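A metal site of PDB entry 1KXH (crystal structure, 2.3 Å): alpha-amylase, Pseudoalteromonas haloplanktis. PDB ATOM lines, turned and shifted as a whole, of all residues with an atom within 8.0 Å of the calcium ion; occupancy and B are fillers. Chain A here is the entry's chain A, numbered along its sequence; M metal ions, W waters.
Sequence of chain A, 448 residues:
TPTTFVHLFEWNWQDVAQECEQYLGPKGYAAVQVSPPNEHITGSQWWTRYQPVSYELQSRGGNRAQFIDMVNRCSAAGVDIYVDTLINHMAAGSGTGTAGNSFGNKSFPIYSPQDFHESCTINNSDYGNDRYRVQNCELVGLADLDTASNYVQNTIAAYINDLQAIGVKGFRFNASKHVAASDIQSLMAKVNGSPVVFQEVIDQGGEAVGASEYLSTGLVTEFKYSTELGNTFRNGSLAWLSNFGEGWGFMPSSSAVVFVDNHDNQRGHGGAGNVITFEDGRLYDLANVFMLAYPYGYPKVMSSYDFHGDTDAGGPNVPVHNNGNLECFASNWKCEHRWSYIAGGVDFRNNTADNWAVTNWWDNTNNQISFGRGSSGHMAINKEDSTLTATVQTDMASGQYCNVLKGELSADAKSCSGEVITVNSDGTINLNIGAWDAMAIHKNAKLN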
ATOM      1  N   ILE A  87     -19.461 -14.709   2.410  1.00  0.00           N
ATOM      2  CA  ILE A  87     -18.283 -14.064   2.974  1.00  0.00           C
ATOM      3  C   ILE A  87     -17.168 -13.790   1.953  1.00  0.00           C
ATOM      4  O   ILE A  87     -16.206 -13.096   2.256  1.00  0.00           O
ATOM      5  CB  ILE A  87     -17.667 -14.938   4.082  1.00  0.00           C
ATOM      6  CG1 ILE A  87     -17.231 -16.290   3.494  1.00  0.00           C
ATOM      7  CG2 ILE A  87     -18.674 -15.156   5.214  1.00  0.00           C
ATOM      8  CD1 ILE A  87     -16.291 -17.077   4.399  1.00  0.00           C
ATOM      9  N   ASN A  88     -17.320 -14.293   0.739  1.00  0.00           N
ATOM     10  CA  ASN A  88     -16.248 -14.140  -0.238  1.00  0.00           C
ATOM     11  C   ASN A  88     -16.353 -13.037  -1.272  1.00  0.00           C
ATOM     12  O   ASN A  88     -15.333 -12.473  -1.682  1.00  0.00           O
ATOM     13  CB  ASN A  88     -16.044 -15.471  -0.975  1.00  0.00           C
ATOM     14  CG  ASN A  88     -14.939 -15.420  -2.050  1.00  0.00           C
ATOM     15  OD1 ASN A  88     -13.755 -15.380  -1.732  1.00  0.00           O
ATOM     16  ND2 ASN A  88     -15.345 -15.436  -3.326  1.00  0.00           N
ATOM     17  N   HIS A  89     -17.567 -12.652  -1.633  1.00  0.00           N
ATOM     18  CA  HIS A  89     -17.706 -11.695  -2.718  1.00  0.00           C
ATOM     19  C   HIS A  89     -18.995 -10.905  -2.727  1.00  0.00           C
ATOM     20  O   HIS A  89     -19.895 -11.145  -1.920  1.00  0.00           O
ATOM     21  CB  HIS A  89     -17.665 -12.491  -4.026  1.00  0.00           C
ATOM     22  CG  HIS A  89     -18.643 -13.637  -4.060  1.00  0.00           C
ATOM     23  ND1 HIS A  89     -18.307 -14.913  -3.662  1.00  0.00           N
ATOM     24  CD2 HIS A  89     -19.966 -13.670  -4.360  1.00  0.00           C
ATOM     25  CE1 HIS A  89     -19.382 -15.689  -3.723  1.00  0.00           C
ATOM     26  NE2 HIS A  89     -20.404 -14.955  -4.141  1.00  0.00           N
ATOM     27  N   HIS A 117     -10.077  -7.142  -3.914  1.00  0.00           N
ATOM     28  CA  HIS A 117      -8.764  -7.507  -4.435  1.00  0.00           C
ATOM     29  C   HIS A 117      -8.766  -7.022  -5.881  1.00  0.00           C
ATOM     30  O   HIS A 117      -9.832  -6.872  -6.500  1.00  0.00           O
ATOM     31  CB  HIS A 117      -8.613  -9.035  -4.467  1.00  0.00           C
ATOM     32  CG  HIS A 117      -8.526  -9.669  -3.117  1.00  0.00           C
ATOM     33  ND1 HIS A 117      -9.126 -10.877  -2.823  1.00  0.00           N
ATOM     34  CD2 HIS A 117      -7.868  -9.297  -1.991  1.00  0.00           C
ATOM     35  CE1 HIS A 117      -8.843 -11.226  -1.579  1.00  0.00           C
ATOM     36  NE2 HIS A 117      -8.090 -10.276  -1.051  1.00  0.00           N
ATOM     37  N   ILE A 122     -10.046 -16.708 -11.870  1.00  0.00           N
ATOM     38  CA  ILE A 122      -9.638 -18.014 -11.370  1.00  0.00           C
ATOM     39  C   ILE A 122      -9.867 -18.976 -12.528  1.00  0.00           C
ATOM     40  O   ILE A 122     -10.955 -18.988 -13.107  1.00  0.00           O
ATOM     41  CB  ILE A 122     -10.501 -18.502 -10.185  1.00  0.00           C
ATOM     42  CG1 ILE A 122     -10.390 -17.558  -8.978  1.00  0.00           C
ATOM     43  CG2 ILE A 122     -10.049 -19.898  -9.753  1.00  0.00           C
ATOM     44  CD1 ILE A 122     -11.246 -17.983  -7.779  1.00  0.00           C
ATOM     45  N   TYR A 132      -2.953 -18.989  -4.177  1.00  0.00           N
ATOM     46  CA  TYR A 132      -3.082 -17.533  -4.188  1.00  0.00           C
ATOM     47  C   TYR A 132      -4.177 -17.062  -5.140  1.00  0.00           C
ATOM     48  O   TYR A 132      -4.937 -16.145  -4.802  1.00  0.00           O
ATOM     49  CB  TYR A 132      -1.746 -16.888  -4.566  1.00  0.00           C
ATOM     50  CG  TYR A 132      -1.839 -15.388  -4.765  1.00  0.00           C
ATOM     51  CD1 TYR A 132      -1.656 -14.513  -3.680  1.00  0.00           C
ATOM     52  CD2 TYR A 132      -2.111 -14.838  -6.015  1.00  0.00           C
ATOM     53  CE1 TYR A 132      -1.754 -13.122  -3.856  1.00  0.00           C
ATOM     54  CE2 TYR A 132      -2.219 -13.454  -6.198  1.00  0.00           C
ATOM     55  CZ  TYR A 132      -2.035 -12.601  -5.109  1.00  0.00           C
ATOM     56  OH  TYR A 132      -2.111 -11.237  -5.288  1.00  0.00           O
ATOM     57  N   ARG A 133      -4.236 -17.626  -6.341  1.00  0.00           N
ATOM     58  CA  ARG A 133      -5.258 -17.236  -7.304  1.00  0.00           C
ATOM     59  C   ARG A 133      -6.662 -17.718  -6.892  1.00  0.00           C
ATOM     60  O   ARG A 133      -7.639 -16.999  -7.092  1.00  0.00           O
ATOM     61  CB  ARG A 133      -4.893 -17.708  -8.709  1.00  0.00           C
ATOM     62  CG  ARG A 133      -3.694 -16.960  -9.287  1.00  0.00           C
ATOM     63  CD  ARG A 133      -3.361 -17.402 -10.716  1.00  0.00           C
ATOM     64  NE  ARG A 133      -4.430 -17.067 -11.648  1.00  0.00           N
ATOM     65  CZ  ARG A 133      -4.563 -15.904 -12.283  1.00  0.00           C
ATOM     66  NH1 ARG A 133      -5.583 -15.714 -13.112  1.00  0.00           N
ATOM     67  NH2 ARG A 133      -3.655 -14.946 -12.142  1.00  0.00           N
ATOM     68  N   VAL A 134      -6.738 -18.901  -6.284  1.00  0.00           N
ATOM     69  CA  VAL A 134      -8.017 -19.470  -5.813  1.00  0.00           C
ATOM     70  C   VAL A 134      -8.649 -18.536  -4.757  1.00  0.00           C
ATOM     71  O   VAL A 134      -9.861 -18.305  -4.766  1.00  0.00           O
ATOM     72  CB  VAL A 134      -7.791 -20.902  -5.153  1.00  0.00           C
ATOM     73  CG1 VAL A 134      -9.070 -21.410  -4.461  1.00  0.00           C
ATOM     74  CG2 VAL A 134      -7.355 -21.925  -6.194  1.00  0.00           C
ATOM     75  N   GLN A 135      -7.824 -17.955  -3.894  1.00  0.00           N
ATOM     76  CA  GLN A 135      -8.311 -17.103  -2.807  1.00  0.00           C
ATOM     77  C   GLN A 135      -8.325 -15.590  -3.028  1.00  0.00           C
ATOM     78  O   GLN A 135      -9.011 -14.872  -2.287  1.00  0.00           O
ATOM     79  CB  GLN A 135      -7.596 -17.484  -1.490  1.00  0.00           C
ATOM     80  CG  GLN A 135      -7.851 -18.959  -1.089  1.00  0.00           C
ATOM     81  CD  GLN A 135      -7.103 -19.415   0.148  1.00  0.00           C
ATOM     82  OE1 GLN A 135      -6.074 -18.860   0.513  1.00  0.00           O
ATOM     83  NE2 GLN A 135      -7.626 -20.462   0.815  1.00  0.00           N
ATOM     84  N   ASN A 136      -7.650 -15.105  -4.074  1.00  0.00           N
ATOM     85  CA  ASN A 136      -7.622 -13.668  -4.361  1.00  0.00           C
ATOM     86  C   ASN A 136      -8.259 -13.254  -5.690  1.00  0.00           C
ATOM     87  O   ASN A 136      -8.587 -12.079  -5.879  1.00  0.00           O
ATOM     88  CB  ASN A 136      -6.195 -13.115  -4.267  1.00  0.00           C
ATOM     89  CG  ASN A 136      -5.633 -13.192  -2.862  1.00  0.00           C
ATOM     90  OD1 ASN A 136      -5.825 -12.296  -2.046  1.00  0.00           O
ATOM     91  ND2 ASN A 136      -4.956 -14.299  -2.565  1.00  0.00           N
ATOM     92  N   CYS A 137      -8.406 -14.195  -6.619  1.00  0.00           N
ATOM     93  CA  CYS A 137      -9.029 -13.863  -7.909  1.00  0.00           C
ATOM     94  C   CYS A 137     -10.529 -14.100  -7.873  1.00  0.00           C
ATOM     95  O   CYS A 137     -11.051 -14.674  -6.918  1.00  0.00           O
ATOM     96  CB  CYS A 137      -8.376 -14.636  -9.054  1.00  0.00           C
ATOM     97  SG  CYS A 137      -6.641 -14.133  -9.334  1.00  0.00           S
ATOM     98  N   GLU A 138     -11.222 -13.698  -8.926  1.00  0.00           N
ATOM     99  CA  GLU A 138     -12.660 -13.805  -9.004  1.00  0.00           C
ATOM    100  C   GLU A 138     -13.253 -15.145  -9.423  1.00  0.00           C
ATOM    101  O   GLU A 138     -12.773 -15.796 -10.337  1.00  0.00           O
ATOM    102  CB  GLU A 138     -13.194 -12.693  -9.915  1.00  0.00           C
ATOM    103  CG  GLU A 138     -12.784 -11.297  -9.431  1.00  0.00           C
ATOM    104  CD  GLU A 138     -13.089 -10.185 -10.438  1.00  0.00           C
ATOM    105  OE1 GLU A 138     -13.400 -10.486 -11.613  1.00  0.00           O
ATOM    106  OE2 GLU A 138     -13.000  -9.000 -10.050  1.00  0.00           O
ATOM    107  N   LEU A 139     -14.305 -15.567  -8.704  1.00  0.00           N
ATOM    108  CA  LEU A 139     -15.032 -16.791  -9.014  1.00  0.00           C
ATOM    109  C   LEU A 139     -16.137 -16.334  -9.968  1.00  0.00           C
ATOM    110  O   LEU A 139     -17.000 -15.547  -9.593  1.00  0.00           O
ATOM    111  CB  LEU A 139     -15.648 -17.392  -7.733  1.00  0.00           C
ATOM    112  CG  LEU A 139     -16.532 -18.631  -7.843  1.00  0.00           C
ATOM    113  CD1 LEU A 139     -15.763 -19.800  -8.401  1.00  0.00           C
ATOM    114  CD2 LEU A 139     -17.080 -18.970  -6.462  1.00  0.00           C
ATOM    115  N   LEU A 142     -17.341 -12.666  -9.938  1.00  0.00           N
ATOM    116  CA  LEU A 142     -17.853 -12.089  -8.710  1.00  0.00           C
ATOM    117  C   LEU A 142     -16.763 -11.246  -8.037  1.00  0.00           C
ATOM    118  O   LEU A 142     -15.638 -11.705  -7.874  1.00  0.00           O
ATOM    119  CB  LEU A 142     -18.340 -13.193  -7.780  1.00  0.00           C
ATOM    120  CG  LEU A 142     -19.437 -14.086  -8.388  1.00  0.00           C
ATOM    121  CD1 LEU A 142     -19.556 -15.381  -7.564  1.00  0.00           C
ATOM    122  CD2 LEU A 142     -20.775 -13.335  -8.443  1.00  0.00           C
ATOM    123  N   ALA A 143     -17.098 -10.003  -7.705  1.00  0.00           N
ATOM    124  CA  ALA A 143     -16.142  -9.082  -7.085  1.00  0.00           C
ATOM    125  C   ALA A 143     -15.576  -9.713  -5.814  1.00  0.00           C
ATOM    126  O   ALA A 143     -16.320 -10.038  -4.884  1.00  0.00           O
ATOM    127  CB  ALA A 143     -16.812  -7.757  -6.788  1.00  0.00           C
ATOM    128  N   ASP A 144     -14.265  -9.892  -5.779  1.00  0.00           N
ATOM    129  CA  ASP A 144     -13.619 -10.548  -4.641  1.00  0.00           C
ATOM    130  C   ASP A 144     -13.257  -9.632  -3.469  1.00  0.00           C
ATOM    131  O   ASP A 144     -12.368  -8.787  -3.582  1.00  0.00           O
ATOM    132  CB  ASP A 144     -12.407 -11.348  -5.137  1.00  0.00           C
ATOM    133  CG  ASP A 144     -12.097 -12.578  -4.278  1.00  0.00           C
ATOM    134  OD1 ASP A 144     -12.944 -13.497  -4.182  1.00  0.00           O
ATOM    135  OD2 ASP A 144     -10.996 -12.630  -3.699  1.00  0.00           O
ATOM    136  N   LEU A 145     -13.957  -9.791  -2.350  1.00  0.00           N
ATOM    137  CA  LEU A 145     -13.730  -8.976  -1.152  1.00  0.00           C
ATOM    138  C   LEU A 145     -12.342  -9.161  -0.536  1.00  0.00           C
ATOM    139  O   LEU A 145     -11.808 -10.273  -0.507  1.00  0.00           O
ATOM    140  CB  LEU A 145     -14.783  -9.282  -0.079  1.00  0.00           C
ATOM    141  CG  LEU A 145     -16.185  -8.673  -0.177  1.00  0.00           C
ATOM    142  CD1 LEU A 145     -17.102  -9.317   0.863  1.00  0.00           C
ATOM    143  CD2 LEU A 145     -16.123  -7.175   0.027  1.00  0.00           C
ATOM    144  N   ASP A 146     -11.757  -8.053  -0.087  1.00  0.00           N
ATOM    145  CA  ASP A 146     -10.455  -8.104   0.574  1.00  0.00           C
ATOM    146  C   ASP A 146     -10.756  -8.553   2.024  1.00  0.00           C
ATOM    147  O   ASP A 146     -10.833  -7.743   2.949  1.00  0.00           O
ATOM    148  CB  ASP A 146      -9.790  -6.723   0.540  1.00  0.00           C
ATOM    149  CG  ASP A 146      -8.400  -6.731   1.169  1.00  0.00           C
ATOM    150  OD1 ASP A 146      -7.943  -7.791   1.654  1.00  0.00           O
ATOM    151  OD2 ASP A 146      -7.749  -5.664   1.193  1.00  0.00           O
ATOM    152  N   THR A 147     -10.912  -9.870   2.198  1.00  0.00           N
ATOM    153  CA  THR A 147     -11.250 -10.425   3.501  1.00  0.00           C
ATOM    154  C   THR A 147     -10.161 -10.311   4.562  1.00  0.00           C
ATOM    155  O   THR A 147     -10.355 -10.781   5.672  1.00  0.00           O
ATOM    156  CB  THR A 147     -11.763 -11.887   3.373  1.00  0.00           C
ATOM    157  OG1 THR A 147     -10.814 -12.666   2.649  1.00  0.00           O
ATOM    158  CG2 THR A 147     -13.103 -11.916   2.647  1.00  0.00           C
ATOM    159  N   ALA A 175     -18.795 -20.631  -0.249  1.00  0.00           N
ATOM    160  CA  ALA A 175     -17.540 -20.476  -0.980  1.00  0.00           C
ATOM    161  C   ALA A 175     -16.306 -20.286  -0.091  1.00  0.00           C
ATOM    162  O   ALA A 175     -15.406 -19.509  -0.418  1.00  0.00           O
ATOM    163  CB  ALA A 175     -17.668 -19.306  -1.991  1.00  0.00           C
ATOM    164  N   SER A 176     -16.238 -21.026   0.999  1.00  0.00           N
ATOM    165  CA  SER A 176     -15.130 -20.898   1.947  1.00  0.00           C
ATOM    166  C   SER A 176     -13.719 -21.242   1.463  1.00  0.00           C
ATOM    167  O   SER A 176     -12.745 -20.717   2.003  1.00  0.00           O
ATOM    168  CB  SER A 176     -15.447 -21.704   3.207  1.00  0.00           C
ATOM    169  OG  SER A 176     -16.614 -21.207   3.818  1.00  0.00           O
ATOM    170  N   LYS A 177     -13.590 -22.120   0.465  1.00  0.00           N
ATOM    171  CA  LYS A 177     -12.257 -22.475  -0.012  1.00  0.00           C
ATOM    172  C   LYS A 177     -11.602 -21.257  -0.684  1.00  0.00           C
ATOM    173  O   LYS A 177     -10.366 -21.169  -0.774  1.00  0.00           O
ATOM    174  CB  LYS A 177     -12.314 -23.663  -0.985  1.00  0.00           C
ATOM    175  CG  LYS A 177     -12.720 -23.293  -2.402  1.00  0.00           C
ATOM    176  CD  LYS A 177     -13.144 -24.503  -3.264  1.00  0.00           C
ATOM    177  CE  LYS A 177     -12.009 -25.481  -3.480  1.00  0.00           C
ATOM    178  NZ  LYS A 177     -12.449 -26.582  -4.380  1.00  0.00           N
ATOM    179  N   HIS A 178     -12.443 -20.303  -1.080  1.00  0.00           N
ATOM    180  CA  HIS A 178     -11.969 -19.081  -1.734  1.00  0.00           C
ATOM    181  C   HIS A 178     -11.558 -17.978  -0.748  1.00  0.00           C
ATOM    182  O   HIS A 178     -11.255 -16.857  -1.147  1.00  0.00           O
ATOM    183  CB  HIS A 178     -13.025 -18.597  -2.721  1.00  0.00           C
ATOM    184  CG  HIS A 178     -13.323 -19.584  -3.809  1.00  0.00           C
ATOM    185  ND1 HIS A 178     -12.562 -19.675  -4.957  1.00  0.00           N
ATOM    186  CD2 HIS A 178     -14.281 -20.534  -3.920  1.00  0.00           C
ATOM    187  CE1 HIS A 178     -13.027 -20.643  -5.720  1.00  0.00           C
ATOM    188  NE2 HIS A 178     -14.075 -21.180  -5.114  1.00  0.00           N
ATOM    189  N   VAL A 179     -11.546 -18.315   0.530  1.00  0.00           N
ATOM    190  CA  VAL A 179     -11.127 -17.374   1.568  1.00  0.00           C
ATOM    191  C   VAL A 179     -10.101 -18.093   2.422  1.00  0.00           C
ATOM    192  O   VAL A 179     -10.322 -19.229   2.860  1.00  0.00           O
ATOM    193  CB  VAL A 179     -12.317 -16.927   2.487  1.00  0.00           C
ATOM    194  CG1 VAL A 179     -11.809 -15.963   3.548  1.00  0.00           C
ATOM    195  CG2 VAL A 179     -13.420 -16.278   1.662  1.00  0.00           C
ATOM    196  N   ALA A 180      -8.957 -17.452   2.631  1.00  0.00           N
ATOM    197  CA  ALA A 180      -7.898 -18.031   3.450  1.00  0.00           C
ATOM    198  C   ALA A 180      -8.465 -18.385   4.830  1.00  0.00           C
ATOM    199  O   ALA A 180      -9.166 -17.581   5.438  1.00  0.00           O
ATOM    200  CB  ALA A 180      -6.762 -17.034   3.592  1.00  0.00           C
ATOM    201  N   ASP A 183      -8.115 -15.764   7.418  1.00  0.00           N
ATOM    202  CA  ASP A 183      -9.022 -14.618   7.315  1.00  0.00           C
ATOM    203  C   ASP A 183     -10.296 -14.977   8.080  1.00  0.00           C
ATOM    204  O   ASP A 183     -10.889 -14.117   8.736  1.00  0.00           O
ATOM    205  CB  ASP A 183      -9.403 -14.342   5.858  1.00  0.00           C
ATOM    206  CG  ASP A 183      -8.326 -13.614   5.088  1.00  0.00           C
ATOM    207  OD1 ASP A 183      -8.554 -13.352   3.891  1.00  0.00           O
ATOM    208  OD2 ASP A 183      -7.263 -13.294   5.653  1.00  0.00           O
HETATM  209 CA    CA M   1     -11.543 -14.621  -2.128  1.00  0.00          CA
HETATM  210  O   HOH W   1     -10.474 -13.836  -0.144  1.00  0.00           O
HETATM  211  O   HOH W   2     -11.122 -15.866  -4.361  1.00  0.00           O
HETATM  212  O   HOH W   3     -12.690 -12.725  -1.032  1.00  0.00           O
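Water W3 lies within hydrogen-bond range of O of Leu 145 and O of Asn 88.
Of the 26 residues printed, 4 come within 4 Å of the calcium ion. The nearest printed residue that does not touch the calcium ion is His 117 (4.4 Å).
The side-chain amide nitrogen of Asn 88 sits at hydrogen-bond distance from a ring nitrogen (ND1) of His 89, at 3.0 Å. The backbone NH of Leu 145 is in hydrogen-bond range of the backbone carbonyl oxygen of Asn 88, at 3.1 Å. The backbone carbonyl oxygen of Lys 177 is in hydrogen-bond range of the side-chain amide nitrogen of Gln 135 (3.2 Å). ND1 of His 178 lies within hydrogen-bond range of O of Val 134 (3.0 Å). The backbone carbonyl oxygen (O) of Asp 144 lies within hydrogen-bond range of the backbone NH (N) of His 117.
OD1 of Asn 88 binds the calcium ion (2.4 Å). Water W1 is bound to the calcium ion (2.4 Å). O of His 178 binds the calcium ion (2.5 Å). Water W3 binds the calcium ion. The calcium ion is bound by O of Gln 135, 2.5 Å away. The calcium ion is bound by water W2 (2.6 Å). OD2 of Asp 144 binds the calcium ion (2.6 Å). The side-chain carboxylate (OD1) of Asp 144 binds the calcium ion. The calcium ion has eight donor atoms within binding distance.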
